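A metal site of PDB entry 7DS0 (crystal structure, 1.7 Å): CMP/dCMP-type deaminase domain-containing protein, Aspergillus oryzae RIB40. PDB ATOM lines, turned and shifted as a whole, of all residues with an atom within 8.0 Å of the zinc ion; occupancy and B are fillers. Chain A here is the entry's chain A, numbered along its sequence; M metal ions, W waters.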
ATOM      1  N   VAL A  28     -29.648   4.997 -13.148  1.00  0.00           N
ATOM      2  CA  VAL A  28     -29.476   5.188 -11.712  1.00  0.00           C
ATOM      3  C   VAL A  28     -29.765   6.648 -11.400  1.00  0.00           C
ATOM      4  O   VAL A  28     -29.610   7.527 -12.246  1.00  0.00           O
ATOM      5  CB  VAL A  28     -28.049   4.776 -11.275  1.00  0.00           C
ATOM      6  CG1 VAL A  28     -27.779   5.105  -9.795  1.00  0.00           C
ATOM      7  CG2 VAL A  28     -27.814   3.283 -11.524  1.00  0.00           C
ATOM      8  N   THR A  53     -28.084   8.924 -14.497  1.00  0.00           N
ATOM      9  CA  THR A  53     -27.258   8.369 -15.566  1.00  0.00           C
ATOM     10  C   THR A  53     -27.471   9.122 -16.873  1.00  0.00           C
ATOM     11  O   THR A  53     -28.602   9.256 -17.347  1.00  0.00           O
ATOM     12  CB  THR A  53     -27.584   6.891 -15.723  1.00  0.00           C
ATOM     13  OG1 THR A  53     -27.383   6.236 -14.465  1.00  0.00           O
ATOM     14  CG2 THR A  53     -26.681   6.220 -16.788  1.00  0.00           C
ATOM     15  N   THR A  60     -21.786   9.400 -18.595  1.00  0.00           N
ATOM     16  CA  THR A  60     -21.752   9.879 -17.223  1.00  0.00           C
ATOM     17  C   THR A  60     -22.658   9.035 -16.337  1.00  0.00           C
ATOM     18  O   THR A  60     -23.756   8.656 -16.744  1.00  0.00           O
ATOM     19  CB  THR A  60     -22.190  11.350 -17.119  1.00  0.00           C
ATOM     20  OG1 THR A  60     -23.477  11.505 -17.722  1.00  0.00           O
ATOM     21  CG2 THR A  60     -21.192  12.268 -17.813  1.00  0.00           C
ATOM     22  N   HIS A  61     -22.194   8.760 -15.119  1.00  0.00           N
ATOM     23  CA  HIS A  61     -22.959   8.021 -14.136  1.00  0.00           C
ATOM     24  C   HIS A  61     -23.772   8.984 -13.269  1.00  0.00           C
ATOM     25  O   HIS A  61     -23.526  10.200 -13.243  1.00  0.00           O
ATOM     26  CB  HIS A  61     -22.017   7.186 -13.268  1.00  0.00           C
ATOM     27  CG  HIS A  61     -21.514   5.946 -13.962  1.00  0.00           C
ATOM     28  ND1 HIS A  61     -20.861   4.929 -13.302  1.00  0.00           N
ATOM     29  CD2 HIS A  61     -21.593   5.556 -15.257  1.00  0.00           C
ATOM     30  CE1 HIS A  61     -20.545   3.973 -14.151  1.00  0.00           C
ATOM     31  NE2 HIS A  61     -20.985   4.327 -15.349  1.00  0.00           N
ATOM     32  N   ALA A  62     -24.762   8.429 -12.549  1.00  0.00           N
ATOM     33  CA  ALA A  62     -25.627   9.247 -11.698  1.00  0.00           C
ATOM     34  C   ALA A  62     -24.826  10.017 -10.660  1.00  0.00           C
ATOM     35  O   ALA A  62     -25.011  11.228 -10.490  1.00  0.00           O
ATOM     36  CB  ALA A  62     -26.677   8.367 -11.022  1.00  0.00           C
ATOM     37  N   GLU A  63     -23.948   9.322  -9.923  1.00  0.00           N
ATOM     38  CA  GLU A  63     -23.167   9.978  -8.873  1.00  0.00           C
ATOM     39  C   GLU A  63     -22.265  11.053  -9.458  1.00  0.00           C
ATOM     40  O   GLU A  63     -22.081  12.120  -8.857  1.00  0.00           O
ATOM     41  CB  GLU A  63     -22.308   8.941  -8.142  1.00  0.00           C
ATOM     42  CG  GLU A  63     -23.119   7.753  -7.599  1.00  0.00           C
ATOM     43  CD  GLU A  63     -23.171   6.588  -8.585  1.00  0.00           C
ATOM     44  OE1 GLU A  63     -23.691   6.768  -9.711  1.00  0.00           O
ATOM     45  OE2 GLU A  63     -22.684   5.489  -8.234  1.00  0.00           O
ATOM     46  N   GLN A  64     -21.691  10.764 -10.635  1.00  0.00           N
ATOM     47  CA  GLN A  64     -20.840  11.700 -11.343  1.00  0.00           C
ATOM     48  C   GLN A  64     -21.617  12.955 -11.739  1.00  0.00           C
ATOM     49  O   GLN A  64     -21.142  14.070 -11.529  1.00  0.00           O
ATOM     50  CB  GLN A  64     -20.265  10.990 -12.572  1.00  0.00           C
ATOM     51  CG  GLN A  64     -19.388  11.816 -13.485  1.00  0.00           C
ATOM     52  CD  GLN A  64     -18.937  11.025 -14.693  1.00  0.00           C
ATOM     53  OE1 GLN A  64     -19.437   9.921 -14.935  1.00  0.00           O
ATOM     54  NE2 GLN A  64     -17.989  11.577 -15.464  1.00  0.00           N
ATOM     55  N   VAL A  97     -28.107   6.700  -3.547  1.00  0.00           N
ATOM     56  CA  VAL A  97     -27.970   6.253  -4.934  1.00  0.00           C
ATOM     57  C   VAL A  97     -28.683   4.914  -5.056  1.00  0.00           C
ATOM     58  O   VAL A  97     -28.607   4.085  -4.152  1.00  0.00           O
ATOM     59  CB  VAL A  97     -26.470   6.185  -5.321  1.00  0.00           C
ATOM     60  CG1 VAL A  97     -25.719   5.184  -4.442  1.00  0.00           C
ATOM     61  CG2 VAL A  97     -26.266   5.888  -6.802  1.00  0.00           C
ATOM     62  N   MET A  99     -28.240   2.263  -6.810  1.00  0.00           N
ATOM     63  CA  MET A  99     -27.316   1.138  -6.912  1.00  0.00           C
ATOM     64  C   MET A  99     -25.980   1.505  -6.282  1.00  0.00           C
ATOM     65  O   MET A  99     -25.535   2.652  -6.345  1.00  0.00           O
ATOM     66  CB  MET A  99     -27.105   0.741  -8.375  1.00  0.00           C
ATOM     67  CG  MET A  99     -26.220  -0.466  -8.602  1.00  0.00           C
ATOM     68  SD  MET A  99     -26.132  -0.861 -10.368  1.00  0.00           S
ATOM     69  CE  MET A  99     -27.856  -0.627 -10.828  1.00  0.00           C
ATOM     70  N   GLU A 100     -25.332   0.497  -5.683  1.00  0.00           N
ATOM     71  CA  GLU A 100     -23.968   0.587  -5.177  1.00  0.00           C
ATOM     72  C   GLU A 100     -23.055   1.324  -6.153  1.00  0.00           C
ATOM     73  O   GLU A 100     -22.993   0.948  -7.340  1.00  0.00           O
ATOM     74  CB  GLU A 100     -23.427  -0.822  -4.924  1.00  0.00           C
ATOM     75  CG  GLU A 100     -22.002  -0.877  -4.396  1.00  0.00           C
ATOM     76  CD  GLU A 100     -21.533  -2.298  -4.187  1.00  0.00           C
ATOM     77  OE1 GLU A 100     -22.113  -3.229  -4.816  1.00  0.00           O
ATOM     78  OE2 GLU A 100     -20.604  -2.505  -3.399  1.00  0.00           O
ATOM     79  N   PRO A 101     -22.334   2.363  -5.705  1.00  0.00           N
ATOM     80  CA  PRO A 101     -21.396   3.062  -6.612  1.00  0.00           C
ATOM     81  C   PRO A 101     -20.343   2.123  -7.163  1.00  0.00           C
ATOM     82  O   PRO A 101     -19.850   1.231  -6.468  1.00  0.00           O
ATOM     83  CB  PRO A 101     -20.763   4.131  -5.701  1.00  0.00           C
ATOM     84  CG  PRO A 101     -21.752   4.349  -4.614  1.00  0.00           C
ATOM     85  CD  PRO A 101     -22.448   3.016  -4.397  1.00  0.00           C
ATOM     86  N   CYS A 102     -20.015   2.333  -8.440  1.00  0.00           N
ATOM     87  CA  CYS A 102     -19.049   1.479  -9.115  1.00  0.00           C
ATOM     88  C   CYS A 102     -17.648   1.686  -8.574  1.00  0.00           C
ATOM     89  O   CYS A 102     -17.243   2.809  -8.244  1.00  0.00           O
ATOM     90  CB  CYS A 102     -19.101   1.727 -10.640  1.00  0.00           C
ATOM     91  SG  CYS A 102     -18.521   3.396 -11.184  1.00  0.00           S
ATOM     92  N   GLY A 103     -16.906   0.578  -8.466  1.00  0.00           N
ATOM     93  CA  GLY A 103     -15.513   0.583  -8.042  1.00  0.00           C
ATOM     94  C   GLY A 103     -14.560   0.490  -9.218  1.00  0.00           C
ATOM     95  O   GLY A 103     -13.361   0.757  -9.082  1.00  0.00           O
ATOM     96  N   LYS A 104     -15.074   0.082 -10.371  1.00  0.00           N
ATOM     97  CA  LYS A 104     -14.320   0.052 -11.620  1.00  0.00           C
ATOM     98  C   LYS A 104     -15.299   0.306 -12.747  1.00  0.00           C
ATOM     99  O   LYS A 104     -16.484  -0.003 -12.607  1.00  0.00           O
ATOM    100  CB  LYS A 104     -13.596  -1.298 -11.850  1.00  0.00           C
ATOM    101  CG  LYS A 104     -12.645  -1.729 -10.723  1.00  0.00           C
ATOM    102  CD  LYS A 104     -12.162  -3.169 -10.866  1.00  0.00           C
ATOM    103  CE  LYS A 104     -11.113  -3.513  -9.813  1.00  0.00           C
ATOM    104  NZ  LYS A 104     -11.470  -2.974  -8.455  1.00  0.00           N
ATOM    105  N   ARG A 105     -14.825   0.893 -13.834  1.00  0.00           N
ATOM    106  CA  ARG A 105     -15.675   1.086 -15.015  1.00  0.00           C
ATOM    107  C   ARG A 105     -15.016   0.422 -16.206  1.00  0.00           C
ATOM    108  O   ARG A 105     -13.805   0.566 -16.412  1.00  0.00           O
ATOM    109  CB  ARG A 105     -15.936   2.579 -15.283  1.00  0.00           C
ATOM    110  CG  ARG A 105     -16.855   3.197 -14.235  1.00  0.00           C
ATOM    111  CD  ARG A 105     -17.046   4.708 -14.446  1.00  0.00           C
ATOM    112  NE  ARG A 105     -17.708   4.976 -15.722  1.00  0.00           N
ATOM    113  CZ  ARG A 105     -18.174   6.168 -16.090  1.00  0.00           C
ATOM    114  NH1 ARG A 105     -18.755   6.298 -17.272  1.00  0.00           N
ATOM    115  NH2 ARG A 105     -18.052   7.220 -15.269  1.00  0.00           N
ATOM    116  N   ASN A 109     -13.005   4.928 -17.307  1.00  0.00           N
ATOM    117  CA  ASN A 109     -13.268   6.209 -16.669  1.00  0.00           C
ATOM    118  C   ASN A 109     -13.154   6.066 -15.161  1.00  0.00           C
ATOM    119  O   ASN A 109     -13.273   4.968 -14.600  1.00  0.00           O
ATOM    120  CB  ASN A 109     -14.657   6.723 -17.062  1.00  0.00           C
ATOM    121  CG  ASN A 109     -14.751   7.085 -18.537  1.00  0.00           C
ATOM    122  OD1 ASN A 109     -13.739   7.288 -19.204  1.00  0.00           O
ATOM    123  ND2 ASN A 109     -15.976   7.147 -19.063  1.00  0.00           N
ATOM    124  N   LEU A 110     -12.894   7.184 -14.487  1.00  0.00           N
ATOM    125  CA  LEU A 110     -12.713   7.143 -13.042  1.00  0.00           C
ATOM    126  C   LEU A 110     -13.992   6.631 -12.362  1.00  0.00           C
ATOM    127  O   LEU A 110     -15.082   7.144 -12.624  1.00  0.00           O
ATOM    128  CB  LEU A 110     -12.366   8.533 -12.516  1.00  0.00           C
ATOM    129  CG  LEU A 110     -11.999   8.569 -11.025  1.00  0.00           C
ATOM    130  CD1 LEU A 110     -10.610   7.951 -10.827  1.00  0.00           C
ATOM    131  CD2 LEU A 110     -12.039   9.991 -10.531  1.00  0.00           C
ATOM    132  N   PRO A 111     -13.892   5.630 -11.483  1.00  0.00           N
ATOM    133  CA  PRO A 111     -15.107   5.056 -10.890  1.00  0.00           C
ATOM    134  C   PRO A 111     -15.725   5.999  -9.873  1.00  0.00           C
ATOM    135  O   PRO A 111     -15.073   6.878  -9.311  1.00  0.00           O
ATOM    136  CB  PRO A 111     -14.609   3.761 -10.223  1.00  0.00           C
ATOM    137  CG  PRO A 111     -13.149   3.958 -10.023  1.00  0.00           C
ATOM    138  CD  PRO A 111     -12.673   4.871 -11.123  1.00  0.00           C
ATOM    139  N   CYS A 112     -17.022   5.792  -9.633  1.00  0.00           N
ATOM    140  CA  CYS A 112     -17.746   6.727  -8.779  1.00  0.00           C
ATOM    141  C   CYS A 112     -17.238   6.699  -7.347  1.00  0.00           C
ATOM    142  O   CYS A 112     -17.253   7.725  -6.661  1.00  0.00           O
ATOM    143  CB  CYS A 112     -19.252   6.418  -8.829  1.00  0.00           C
ATOM    144  SG  CYS A 112     -19.991   6.858 -10.395  1.00  0.00           S
ATOM    145  N   VAL A 113     -16.779   5.529  -6.864  1.00  0.00           N
ATOM    146  CA  VAL A 113     -16.265   5.472  -5.505  1.00  0.00           C
ATOM    147  C   VAL A 113     -15.103   6.462  -5.356  1.00  0.00           C
ATOM    148  O   VAL A 113     -14.974   7.135  -4.323  1.00  0.00           O
ATOM    149  CB  VAL A 113     -15.845   4.035  -5.146  1.00  0.00           C
ATOM    150  CG1 VAL A 113     -14.959   4.020  -3.926  1.00  0.00           C
ATOM    151  CG2 VAL A 113     -17.087   3.161  -4.880  1.00  0.00           C
ATOM    152  N   ARG A 115     -14.635   9.243  -7.222  1.00  0.00           N
ATOM    153  CA  ARG A 115     -15.232  10.579  -7.227  1.00  0.00           C
ATOM    154  C   ARG A 115     -15.777  10.928  -5.854  1.00  0.00           C
ATOM    155  O   ARG A 115     -15.733  12.090  -5.445  1.00  0.00           O
ATOM    156  CB  ARG A 115     -16.354  10.667  -8.272  1.00  0.00           C
ATOM    157  CG  ARG A 115     -15.874  10.471  -9.719  1.00  0.00           C
ATOM    158  CD  ARG A 115     -16.971  10.723 -10.767  1.00  0.00           C
ATOM    159  NE  ARG A 115     -16.615  10.029 -12.020  1.00  0.00           N
ATOM    160  CZ  ARG A 115     -15.824  10.536 -12.967  1.00  0.00           C
ATOM    161  NH1 ARG A 115     -15.330  11.764 -12.855  1.00  0.00           N
ATOM    162  NH2 ARG A 115     -15.534   9.804 -14.037  1.00  0.00           N
ATOM    163  N   ILE A 116     -16.294   9.926  -5.136  1.00  0.00           N
ATOM    164  CA  ILE A 116     -16.835  10.169  -3.798  1.00  0.00           C
ATOM    165  C   ILE A 116     -15.706  10.373  -2.797  1.00  0.00           C
ATOM    166  O   ILE A 116     -15.705  11.328  -2.003  1.00  0.00           O
ATOM    167  CB  ILE A 116     -17.751   8.998  -3.390  1.00  0.00           C
ATOM    168  CG1 ILE A 116     -19.072   9.074  -4.150  1.00  0.00           C
ATOM    169  CG2 ILE A 116     -18.020   9.001  -1.859  1.00  0.00           C
ATOM    170  CD1 ILE A 116     -19.800   7.728  -4.247  1.00  0.00           C
ATOM    171  N   GLU A 136     -24.097  -3.922  -6.721  1.00  0.00           N
ATOM    172  CA  GLU A 136     -23.811  -3.981  -8.152  1.00  0.00           C
ATOM    173  C   GLU A 136     -24.077  -5.386  -8.675  1.00  0.00           C
ATOM    174  O   GLU A 136     -23.482  -6.351  -8.168  1.00  0.00           O
ATOM    175  CB  GLU A 136     -22.354  -3.579  -8.399  1.00  0.00           C
ATOM    176  CG  GLU A 136     -22.051  -3.186  -9.830  1.00  0.00           C
ATOM    177  CD  GLU A 136     -20.821  -2.293  -9.948  1.00  0.00           C
ATOM    178  OE1 GLU A 136     -19.778  -2.604  -9.315  1.00  0.00           O
ATOM    179  OE2 GLU A 136     -20.890  -1.280 -10.663  1.00  0.00           O
HETATM  180 ZN    ZN M   1     -20.326   4.772 -11.339  1.00  0.00          ZN
HETATM  181  O   HOH W   1     -22.128   3.913 -10.167  1.00  0.00           O
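The guanidinium group (NE) of Arg 105 sits at hydrogen-bond distance from a ring nitrogen (NE2) of His 61 (3.4 Å). The backbone NH of His 61 is in hydrogen-bond range of the side-chain amide oxygen of Gln 64, at 3.0 Å. The backbone carbonyl oxygen of Cys 102 sits at hydrogen-bond distance from the backbone NH of Val 113, 3.1 Å away. The side-chain sulfur (SG) of Cys 112 lies close to the side-chain carboxylate (OE2) of Glu 63 (3.7 Å).
Glu 63 touches the zinc ion (OE2 to ZN, 3.96 Å). Four residues have an atom within 4 Å of the zinc ion: His 61, Glu 63, Cys 102 and Cys 112.
ND1 of His 61 binds the zinc ion. The side-chain sulfur (SG) of Cys 102 is bound to the zinc ion (2.3 Å). The side-chain sulfur (SG) of Cys 112 binds the zinc ion (2.3 Å). Water W1 binds the zinc ion, 2.3 Å away. The zinc ion has four donor atoms within binding distance.
Water W1 lies within hydrogen-bond range of OE2 of Glu 63 and N of Cys 102.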
